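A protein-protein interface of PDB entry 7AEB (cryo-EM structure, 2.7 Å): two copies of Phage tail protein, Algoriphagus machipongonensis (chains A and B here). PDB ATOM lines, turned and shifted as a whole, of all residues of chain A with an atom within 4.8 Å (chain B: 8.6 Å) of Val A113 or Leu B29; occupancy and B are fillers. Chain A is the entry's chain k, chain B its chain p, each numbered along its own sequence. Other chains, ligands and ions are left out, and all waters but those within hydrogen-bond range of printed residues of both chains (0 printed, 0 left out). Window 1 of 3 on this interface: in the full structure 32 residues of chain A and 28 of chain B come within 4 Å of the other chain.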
ATOM      1  N   TYR A  71     -11.430 -11.777 -20.748  1.00  0.00           N
ATOM      2  CA  TYR A  71     -11.298 -10.828 -21.868  1.00  0.00           C
ATOM      3  C   TYR A  71     -10.030 -11.028 -22.679  1.00  0.00           C
ATOM      4  O   TYR A  71     -10.049 -11.009 -23.916  1.00  0.00           O
ATOM      5  CB  TYR A  71     -11.267  -9.364 -21.401  1.00  0.00           C
ATOM      6  CG  TYR A  71     -12.577  -8.644 -21.114  1.00  0.00           C
ATOM      7  CD1 TYR A  71     -12.499  -7.301 -20.795  1.00  0.00           C
ATOM      8  CD2 TYR A  71     -13.821  -9.253 -21.185  1.00  0.00           C
ATOM      9  CE1 TYR A  71     -13.618  -6.580 -20.566  1.00  0.00           C
ATOM     10  CE2 TYR A  71     -14.948  -8.505 -20.956  1.00  0.00           C
ATOM     11  CZ  TYR A  71     -14.838  -7.166 -20.650  1.00  0.00           C
ATOM     12  OH  TYR A  71     -15.948  -6.414 -20.435  1.00  0.00           O
ATOM     13  N   PHE A  72      -8.923 -11.204 -21.973  1.00  0.00           N
ATOM     14  CA  PHE A  72      -7.639 -11.409 -22.600  1.00  0.00           C
ATOM     15  C   PHE A  72      -7.642 -12.698 -23.377  1.00  0.00           C
ATOM     16  O   PHE A  72      -7.166 -12.744 -24.507  1.00  0.00           O
ATOM     17  CB  PHE A  72      -6.496 -11.395 -21.604  1.00  0.00           C
ATOM     18  CG  PHE A  72      -5.170 -11.581 -22.262  1.00  0.00           C
ATOM     19  CD1 PHE A  72      -4.578 -10.544 -22.946  1.00  0.00           C
ATOM     20  CD2 PHE A  72      -4.523 -12.793 -22.221  1.00  0.00           C
ATOM     21  CE1 PHE A  72      -3.374 -10.718 -23.572  1.00  0.00           C
ATOM     22  CE2 PHE A  72      -3.323 -12.968 -22.847  1.00  0.00           C
ATOM     23  CZ  PHE A  72      -2.748 -11.932 -23.522  1.00  0.00           C
ATOM     24  N   TYR A  75      -9.456 -12.414 -26.724  1.00  0.00           N
ATOM     25  CA  TYR A  75      -8.666 -11.562 -27.610  1.00  0.00           C
ATOM     26  C   TYR A  75      -7.484 -12.336 -28.185  1.00  0.00           C
ATOM     27  O   TYR A  75      -7.163 -12.261 -29.371  1.00  0.00           O
ATOM     28  CB  TYR A  75      -8.181 -10.322 -26.880  1.00  0.00           C
ATOM     29  CG  TYR A  75      -7.500  -9.328 -27.775  1.00  0.00           C
ATOM     30  CD1 TYR A  75      -8.277  -8.448 -28.503  1.00  0.00           C
ATOM     31  CD2 TYR A  75      -6.132  -9.294 -27.891  1.00  0.00           C
ATOM     32  CE1 TYR A  75      -7.708  -7.544 -29.334  1.00  0.00           C
ATOM     33  CE2 TYR A  75      -5.552  -8.381 -28.735  1.00  0.00           C
ATOM     34  CZ  TYR A  75      -6.340  -7.509 -29.454  1.00  0.00           C
ATOM     35  OH  TYR A  75      -5.770  -6.601 -30.293  1.00  0.00           O
ATOM     36  N   LEU A 111     -12.314  -6.345 -31.090  1.00  0.00           N
ATOM     37  CA  LEU A 111     -11.502  -5.314 -31.731  1.00  0.00           C
ATOM     38  C   LEU A 111     -10.404  -4.742 -30.817  1.00  0.00           C
ATOM     39  O   LEU A 111      -9.274  -4.558 -31.225  1.00  0.00           O
ATOM     40  CB  LEU A 111     -12.430  -4.215 -32.234  1.00  0.00           C
ATOM     41  CG  LEU A 111     -11.943  -2.998 -32.990  1.00  0.00           C
ATOM     42  CD1 LEU A 111     -13.093  -2.483 -33.821  1.00  0.00           C
ATOM     43  CD2 LEU A 111     -11.495  -1.923 -32.028  1.00  0.00           C
ATOM     44  N   LYS A 112     -10.753  -4.470 -29.561  1.00  0.00           N
ATOM     45  CA  LYS A 112      -9.794  -3.925 -28.576  1.00  0.00           C
ATOM     46  C   LYS A 112     -10.207  -4.297 -27.155  1.00  0.00           C
ATOM     47  O   LYS A 112     -11.413  -4.492 -26.895  1.00  0.00           O
ATOM     48  CB  LYS A 112      -9.652  -2.407 -28.735  1.00  0.00           C
ATOM     49  CG  LYS A 112     -10.937  -1.610 -28.555  1.00  0.00           C
ATOM     50  CD  LYS A 112     -10.729  -0.112 -28.634  1.00  0.00           C
ATOM     51  CE  LYS A 112     -10.125   0.335 -29.949  1.00  0.00           C
ATOM     52  NZ  LYS A 112      -9.930   1.803 -29.991  1.00  0.00           N
ATOM     53  N   VAL A 113      -9.195  -4.438 -26.308  1.00  0.00           N
ATOM     54  CA  VAL A 113      -9.316  -4.677 -24.875  1.00  0.00           C
ATOM     55  C   VAL A 113      -8.566  -3.567 -24.148  1.00  0.00           C
ATOM     56  O   VAL A 113      -7.388  -3.331 -24.403  1.00  0.00           O
ATOM     57  CB  VAL A 113      -8.778  -6.070 -24.478  1.00  0.00           C
ATOM     58  CG1 VAL A 113      -8.887  -6.278 -22.968  1.00  0.00           C
ATOM     59  CG2 VAL A 113      -9.584  -7.135 -25.181  1.00  0.00           C
ATOM     60  N   GLN A 114      -9.281  -2.820 -23.293  1.00  0.00           N
ATOM     61  CA  GLN A 114      -8.681  -1.691 -22.521  1.00  0.00           C
ATOM     62  C   GLN A 114      -8.619  -1.968 -21.017  1.00  0.00           C
ATOM     63  O   GLN A 114      -9.628  -2.280 -20.397  1.00  0.00           O
ATOM     64  CB  GLN A 114      -9.356  -0.354 -22.822  1.00  0.00           C
ATOM     65  CG  GLN A 114      -9.076   0.108 -24.242  1.00  0.00           C
ATOM     66  CD  GLN A 114      -9.491   1.524 -24.536  1.00  0.00           C
ATOM     67  OE1 GLN A 114     -10.450   2.036 -23.979  1.00  0.00           O
ATOM     68  NE2 GLN A 114      -8.769   2.170 -25.436  1.00  0.00           N
ATOM     69  N   SER A 115      -7.420  -1.847 -20.478  1.00  0.00           N
ATOM     70  CA  SER A 115      -7.157  -1.986 -19.045  1.00  0.00           C
ATOM     71  C   SER A 115      -7.345  -0.674 -18.296  1.00  0.00           C
ATOM     72  O   SER A 115      -7.442   0.406 -18.894  1.00  0.00           O
ATOM     73  CB  SER A 115      -5.758  -2.510 -18.796  1.00  0.00           C
ATOM     74  OG  SER A 115      -5.602  -3.803 -19.292  1.00  0.00           O
ATOM     75  N   SER A 129     -12.626  -2.849 -19.962  1.00  0.00           N
ATOM     76  CA  SER A 129     -13.612  -2.825 -21.043  1.00  0.00           C
ATOM     77  C   SER A 129     -13.172  -3.442 -22.370  1.00  0.00           C
ATOM     78  O   SER A 129     -11.988  -3.551 -22.700  1.00  0.00           O
ATOM     79  CB  SER A 129     -14.021  -1.401 -21.312  1.00  0.00           C
ATOM     80  OG  SER A 129     -12.973  -0.660 -21.823  1.00  0.00           O
ATOM     81  N   MET A 130     -14.171  -3.840 -23.150  1.00  0.00           N
ATOM     82  CA  MET A 130     -13.985  -4.458 -24.460  1.00  0.00           C
ATOM     83  C   MET A 130     -14.885  -3.889 -25.562  1.00  0.00           C
ATOM     84  O   MET A 130     -16.064  -3.602 -25.346  1.00  0.00           O
ATOM     85  CB  MET A 130     -14.222  -5.963 -24.302  1.00  0.00           C
ATOM     86  CG  MET A 130     -14.164  -6.797 -25.565  1.00  0.00           C
ATOM     87  SD  MET A 130     -14.445  -8.552 -25.248  1.00  0.00           S
ATOM     88  CE  MET A 130     -12.848  -9.137 -24.821  1.00  0.00           C
ATOM     89  N   GLY B  26      -2.233   3.794 -20.019  1.00  0.00           N
ATOM     90  CA  GLY B  26      -1.965   3.395 -21.417  1.00  0.00           C
ATOM     91  C   GLY B  26      -1.797   1.886 -21.692  1.00  0.00           C
ATOM     92  O   GLY B  26      -1.360   1.497 -22.774  1.00  0.00           O
ATOM     93  N   LEU B  27      -2.177   1.024 -20.762  1.00  0.00           N
ATOM     94  CA  LEU B  27      -2.033  -0.425 -20.957  1.00  0.00           C
ATOM     95  C   LEU B  27      -3.130  -1.039 -21.859  1.00  0.00           C
ATOM     96  O   LEU B  27      -3.942  -1.847 -21.413  1.00  0.00           O
ATOM     97  CB  LEU B  27      -2.053  -1.078 -19.563  1.00  0.00           C
ATOM     98  CG  LEU B  27      -0.922  -0.603 -18.562  1.00  0.00           C
ATOM     99  CD1 LEU B  27      -1.173  -1.185 -17.183  1.00  0.00           C
ATOM    100  CD2 LEU B  27       0.440  -1.067 -19.059  1.00  0.00           C
ATOM    101  N   ASP B  28      -3.119  -0.638 -23.133  1.00  0.00           N
ATOM    102  CA  ASP B  28      -4.097  -1.025 -24.165  1.00  0.00           C
ATOM    103  C   ASP B  28      -3.579  -1.985 -25.248  1.00  0.00           C
ATOM    104  O   ASP B  28      -2.384  -2.029 -25.532  1.00  0.00           O
ATOM    105  CB  ASP B  28      -4.597   0.220 -24.882  1.00  0.00           C
ATOM    106  CG  ASP B  28      -5.376   1.173 -24.019  1.00  0.00           C
ATOM    107  OD1 ASP B  28      -6.232   0.739 -23.293  1.00  0.00           O
ATOM    108  OD2 ASP B  28      -5.105   2.352 -24.090  1.00  0.00           O
ATOM    109  N   LEU B  29      -4.510  -2.714 -25.879  1.00  0.00           N
ATOM    110  CA  LEU B  29      -4.262  -3.622 -27.015  1.00  0.00           C
ATOM    111  C   LEU B  29      -5.247  -3.295 -28.149  1.00  0.00           C
ATOM    112  O   LEU B  29      -6.437  -3.148 -27.878  1.00  0.00           O
ATOM    113  CB  LEU B  29      -4.504  -5.074 -26.566  1.00  0.00           C
ATOM    114  CG  LEU B  29      -3.632  -5.616 -25.395  1.00  0.00           C
ATOM    115  CD1 LEU B  29      -4.172  -6.939 -24.932  1.00  0.00           C
ATOM    116  CD2 LEU B  29      -2.229  -5.801 -25.835  1.00  0.00           C
ATOM    117  N   GLU B  30      -4.801  -3.233 -29.415  1.00  0.00           N
ATOM    118  CA  GLU B  30      -5.736  -2.915 -30.514  1.00  0.00           C
ATOM    119  C   GLU B  30      -5.465  -3.642 -31.848  1.00  0.00           C
ATOM    120  O   GLU B  30      -4.320  -3.799 -32.267  1.00  0.00           O
ATOM    121  CB  GLU B  30      -5.728  -1.405 -30.733  1.00  0.00           C
ATOM    122  CG  GLU B  30      -6.698  -0.886 -31.756  1.00  0.00           C
ATOM    123  CD  GLU B  30      -6.658   0.604 -31.846  1.00  0.00           C
ATOM    124  OE1 GLU B  30      -6.014   1.209 -31.038  1.00  0.00           O
ATOM    125  OE2 GLU B  30      -7.227   1.142 -32.758  1.00  0.00           O
ATOM    126  N   THR B  31      -6.535  -4.083 -32.524  1.00  0.00           N
ATOM    127  CA  THR B  31      -6.437  -4.769 -33.828  1.00  0.00           C
ATOM    128  C   THR B  31      -7.276  -4.080 -34.918  1.00  0.00           C
ATOM    129  O   THR B  31      -8.416  -3.688 -34.669  1.00  0.00           O
ATOM    130  CB  THR B  31      -6.880  -6.253 -33.707  1.00  0.00           C
ATOM    131  OG1 THR B  31      -6.067  -6.911 -32.745  1.00  0.00           O
ATOM    132  CG2 THR B  31      -6.705  -6.989 -35.033  1.00  0.00           C
ATOM    133  N   GLU B  32      -6.712  -3.962 -36.124  1.00  0.00           N
ATOM    134  CA  GLU B  32      -7.388  -3.391 -37.298  1.00  0.00           C
ATOM    135  C   GLU B  32      -8.390  -4.338 -37.956  1.00  0.00           C
ATOM    136  O   GLU B  32      -8.307  -5.557 -37.801  1.00  0.00           O
ATOM    137  CB  GLU B  32      -6.361  -3.002 -38.352  1.00  0.00           C
ATOM    138  CG  GLU B  32      -5.466  -1.882 -37.966  1.00  0.00           C
ATOM    139  CD  GLU B  32      -6.207  -0.607 -37.911  1.00  0.00           C
ATOM    140  OE1 GLU B  32      -7.020  -0.388 -38.766  1.00  0.00           O
ATOM    141  OE2 GLU B  32      -5.987   0.162 -37.009  1.00  0.00           O
ATOM    142  N   GLN B  53      -1.805  -5.580 -35.863  1.00  0.00           N
ATOM    143  CA  GLN B  53      -1.961  -5.108 -34.481  1.00  0.00           C
ATOM    144  C   GLN B  53      -1.125  -3.881 -34.083  1.00  0.00           C
ATOM    145  O   GLN B  53      -0.055  -3.632 -34.639  1.00  0.00           O
ATOM    146  CB  GLN B  53      -1.644  -6.259 -33.544  1.00  0.00           C
ATOM    147  CG  GLN B  53      -2.577  -7.434 -33.733  1.00  0.00           C
ATOM    148  CD  GLN B  53      -2.286  -8.568 -32.808  1.00  0.00           C
ATOM    149  OE1 GLN B  53      -1.218  -8.615 -32.194  1.00  0.00           O
ATOM    150  NE2 GLN B  53      -3.219  -9.498 -32.700  1.00  0.00           N
ATOM    151  N   LYS B  54      -1.638  -3.148 -33.089  1.00  0.00           N
ATOM    152  CA  LYS B  54      -1.033  -1.957 -32.481  1.00  0.00           C
ATOM    153  C   LYS B  54      -0.944  -1.986 -30.958  1.00  0.00           C
ATOM    154  O   LYS B  54      -1.715  -2.670 -30.271  1.00  0.00           O
ATOM    155  CB  LYS B  54      -1.833  -0.721 -32.829  1.00  0.00           C
ATOM    156  CG  LYS B  54      -1.846  -0.335 -34.264  1.00  0.00           C
ATOM    157  CD  LYS B  54      -2.813   0.813 -34.505  1.00  0.00           C
ATOM    158  CE  LYS B  54      -4.253   0.296 -34.574  1.00  0.00           C
ATOM    159  NZ  LYS B  54      -5.239   1.352 -34.954  1.00  0.00           N
ATOM    160  N   PHE B  55      -0.026  -1.174 -30.431  1.00  0.00           N
ATOM    161  CA  PHE B  55       0.095  -0.954 -28.995  1.00  0.00           C
ATOM    162  C   PHE B  55       0.145   0.542 -28.694  1.00  0.00           C
ATOM    163  O   PHE B  55       0.664   1.313 -29.495  1.00  0.00           O
ATOM    164  CB  PHE B  55       1.349  -1.612 -28.452  1.00  0.00           C
ATOM    165  CG  PHE B  55       1.368  -3.069 -28.648  1.00  0.00           C
ATOM    166  CD1 PHE B  55       2.061  -3.618 -29.699  1.00  0.00           C
ATOM    167  CD2 PHE B  55       0.655  -3.896 -27.819  1.00  0.00           C
ATOM    168  CE1 PHE B  55       2.043  -4.956 -29.916  1.00  0.00           C
ATOM    169  CE2 PHE B  55       0.637  -5.239 -28.039  1.00  0.00           C
ATOM    170  CZ  PHE B  55       1.327  -5.769 -29.089  1.00  0.00           C
ATOM    171  N   SER B  56      -0.365   0.947 -27.533  1.00  0.00           N
ATOM    172  CA  SER B  56      -0.297   2.346 -27.086  1.00  0.00           C
ATOM    173  C   SER B  56       0.966   2.631 -26.280  1.00  0.00           C
ATOM    174  O   SER B  56       1.551   1.721 -25.689  1.00  0.00           O
ATOM    175  CB  SER B  56      -1.499   2.703 -26.235  1.00  0.00           C
ATOM    176  OG  SER B  56      -2.690   2.651 -26.968  1.00  0.00           O
ATOM    177  N   TRP B 103       1.151  -6.987 -15.678  1.00  0.00           N
ATOM    178  CA  TRP B 103       1.282  -6.542 -17.055  1.00  0.00           C
ATOM    179  C   TRP B 103       2.761  -6.592 -17.447  1.00  0.00           C
ATOM    180  O   TRP B 103       3.609  -5.922 -16.850  1.00  0.00           O
ATOM    181  CB  TRP B 103       0.744  -5.120 -17.229  1.00  0.00           C
ATOM    182  CG  TRP B 103      -0.740  -4.964 -17.030  1.00  0.00           C
ATOM    183  CD1 TRP B 103      -1.705  -4.948 -17.979  1.00  0.00           C
ATOM    184  CD2 TRP B 103      -1.421  -4.748 -15.784  1.00  0.00           C
ATOM    185  NE1 TRP B 103      -2.920  -4.761 -17.411  1.00  0.00           N
ATOM    186  CE2 TRP B 103      -2.769  -4.631 -16.073  1.00  0.00           C
ATOM    187  CE3 TRP B 103      -1.003  -4.641 -14.474  1.00  0.00           C
ATOM    188  CZ2 TRP B 103      -3.704  -4.413 -15.088  1.00  0.00           C
ATOM    189  CZ3 TRP B 103      -1.917  -4.424 -13.494  1.00  0.00           C
ATOM    190  CH2 TRP B 103      -3.239  -4.311 -13.784  1.00  0.00           C
ATOM    191  N   LYS B 104       3.080  -7.431 -18.422  1.00  0.00           N
ATOM    192  CA  LYS B 104       4.459  -7.614 -18.858  1.00  0.00           C
ATOM    193  C   LYS B 104       4.757  -6.897 -20.166  1.00  0.00           C
ATOM    194  O   LYS B 104       4.144  -7.194 -21.195  1.00  0.00           O
ATOM    195  CB  LYS B 104       4.731  -9.098 -19.004  1.00  0.00           C
ATOM    196  CG  LYS B 104       4.633  -9.848 -17.707  1.00  0.00           C
ATOM    197  CD  LYS B 104       4.874 -11.308 -17.898  1.00  0.00           C
ATOM    198  CE  LYS B 104       4.803 -12.040 -16.589  1.00  0.00           C
ATOM    199  NZ  LYS B 104       5.043 -13.491 -16.761  1.00  0.00           N
ATOM    200  N   HIS B 134       7.087   0.801 -26.705  1.00  0.00           N
ATOM    201  CA  HIS B 134       7.396  -0.606 -26.432  1.00  0.00           C
ATOM    202  C   HIS B 134       6.953  -1.483 -27.593  1.00  0.00           C
ATOM    203  O   HIS B 134       6.347  -0.994 -28.546  1.00  0.00           O
ATOM    204  CB  HIS B 134       6.757  -1.054 -25.122  1.00  0.00           C
ATOM    205  CG  HIS B 134       5.301  -1.069 -25.138  1.00  0.00           C
ATOM    206  ND1 HIS B 134       4.558  -2.187 -25.461  1.00  0.00           N
ATOM    207  CD2 HIS B 134       4.429  -0.081 -24.920  1.00  0.00           C
ATOM    208  CE1 HIS B 134       3.288  -1.870 -25.409  1.00  0.00           C
ATOM    209  NE2 HIS B 134       3.192  -0.586 -25.100  1.00  0.00           N
ATOM    210  N   GLY B 136       5.220  -4.736 -27.147  1.00  0.00           N
ATOM    211  CA  GLY B 136       4.317  -5.829 -26.826  1.00  0.00           C
ATOM    212  C   GLY B 136       3.951  -5.956 -25.364  1.00  0.00           C
ATOM    213  O   GLY B 136       4.767  -5.735 -24.465  1.00  0.00           O
ATOM    214  N   LEU B 137       2.711  -6.388 -25.145  1.00  0.00           N
ATOM    215  CA  LEU B 137       2.104  -6.546 -23.833  1.00  0.00           C
ATOM    216  C   LEU B 137       1.368  -7.871 -23.627  1.00  0.00           C
ATOM    217  O   LEU B 137       0.517  -8.255 -24.422  1.00  0.00           O
ATOM    218  CB  LEU B 137       1.131  -5.364 -23.595  1.00  0.00           C
ATOM    219  CG  LEU B 137       0.202  -5.418 -22.341  1.00  0.00           C
ATOM    220  CD1 LEU B 137       1.006  -5.371 -21.072  1.00  0.00           C
ATOM    221  CD2 LEU B 137      -0.776  -4.224 -22.387  1.00  0.00           C
ATOM    222  N   VAL B 138       1.694  -8.534 -22.521  1.00  0.00           N
ATOM    223  CA  VAL B 138       1.056  -9.777 -22.085  1.00  0.00           C
ATOM    224  C   VAL B 138       0.415  -9.598 -20.702  1.00  0.00           C
ATOM    225  O   VAL B 138       1.021  -9.028 -19.794  1.00  0.00           O
ATOM    226  CB  VAL B 138       2.061 -10.948 -22.074  1.00  0.00           C
ATOM    227  CG1 VAL B 138       1.415 -12.221 -21.547  1.00  0.00           C
ATOM    228  CG2 VAL B 138       2.565 -11.183 -23.477  1.00  0.00           C
ATOM    229  N   ILE B 139      -0.834 -10.043 -20.548  1.00  0.00           N
ATOM    230  CA  ILE B 139      -1.526  -9.878 -19.269  1.00  0.00           C
ATOM    231  C   ILE B 139      -1.717 -11.198 -18.527  1.00  0.00           C
ATOM    232  O   ILE B 139      -2.311 -12.139 -19.050  1.00  0.00           O
ATOM    233  CB  ILE B 139      -2.898  -9.216 -19.475  1.00  0.00           C
ATOM    234  CG1 ILE B 139      -2.689  -7.858 -20.165  1.00  0.00           C
ATOM    235  CG2 ILE B 139      -3.581  -9.017 -18.085  1.00  0.00           C
ATOM    236  CD1 ILE B 139      -3.933  -7.177 -20.658  1.00  0.00           C
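Printed residues of chain A that touch a printed residue of chain B: Phe A72, Tyr A75, Leu A111, Lys A112, Val A113, Gln A114 and Ser A115.
Hydrophobic or aromatic side chains of chain A within 4 Å of the printed part of chain B: Phe A72, Tyr A75 and Leu A111.
Hydrophobic or aromatic side chains of chain B within 4 Å of the printed part of chain A: Trp B103.
Among the printed residues, 12 pairs touch across the chains.
Among the printed residues, Asp or Glu carboxylates within 4 Å of a Lys or Arg side-chain nitrogen of the other chain: Lys A112 with Glu B30 (3.9 Å).
OG1 of Thr B31 is in hydrogen-bond range of OH of Tyr A75 (2.5 Å).
The backbone NH (N) of Thr B31 lies within hydrogen-bond range of the backbone carbonyl oxygen (O) of Leu A111 (3.1 Å).
NZ of Lys A112 is in salt-bridge range of OE2 of Glu B30, at 3.9 Å.
The backbone carbonyl oxygen (O) of Val A113 sits at hydrogen-bond distance from the backbone NH (N) of Leu B29.
OG of Ser A115 lies close to O of Leu B27.
OG of Ser A115 is in hydrogen-bond range of NE1 of Trp B103 (3.4 Å).
Phe A72 touches Ile B139 (CD2 to O, 3.9 Å).
Tyr A75 touches Leu B29 (OH to C, 3.97 Å).
C of Glu B30 touches OH of Tyr A75, at 3.4 Å.
Leu A111 touches Glu B30.
Lys A112 touches Leu B29.
OD1 of Asp B28 touches CG of Gln A114, at 3.1 Å.
No position is printed for both chains.
Of the 12 pairs that touch across the chains among the printed residues, none has its exchanged pair printed and touching as well.
Val A113 touches just one residue of chain B: Leu B29 (3.3 Å).
Of chain A, only Tyr A75 (3.97 Å), Lys A112 (3.4 Å) and Val A113 (3.3 Å) come within 4 Å of Leu B29.
Printed residues of chain B within 4 Å of Leu A111: Glu B30 (3.97 Å) and Thr B31 (3.1 Å).
Printed residues of chain B within 4 Å of Phe A72: Ile B139.
Of the printed residues of chain B, Tyr A75 touches Leu B29, Glu B30 and Thr B31.
Of the printed residues of chain A, Ile B139 touches Phe A72.
Lys B104 touches none of the printed residues of chain A.
Phe B55 touches none of the printed residues of chain A.
The nearest residue of chain B that does not touch Val A113 is Asp B28 (4.03 Å).
The nearest residue of chain A that does not touch Leu B29 is Phe A72 (4.1 Å).
The backbone NH of Gln A114 sits at hydrogen-bond distance from the backbone carbonyl oxygen of Ser A129 (2.9 Å).
The side-chain amino group of Lys B54 lies within salt-bridge range of the side-chain carboxylate of Glu B30 (3.0 Å).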
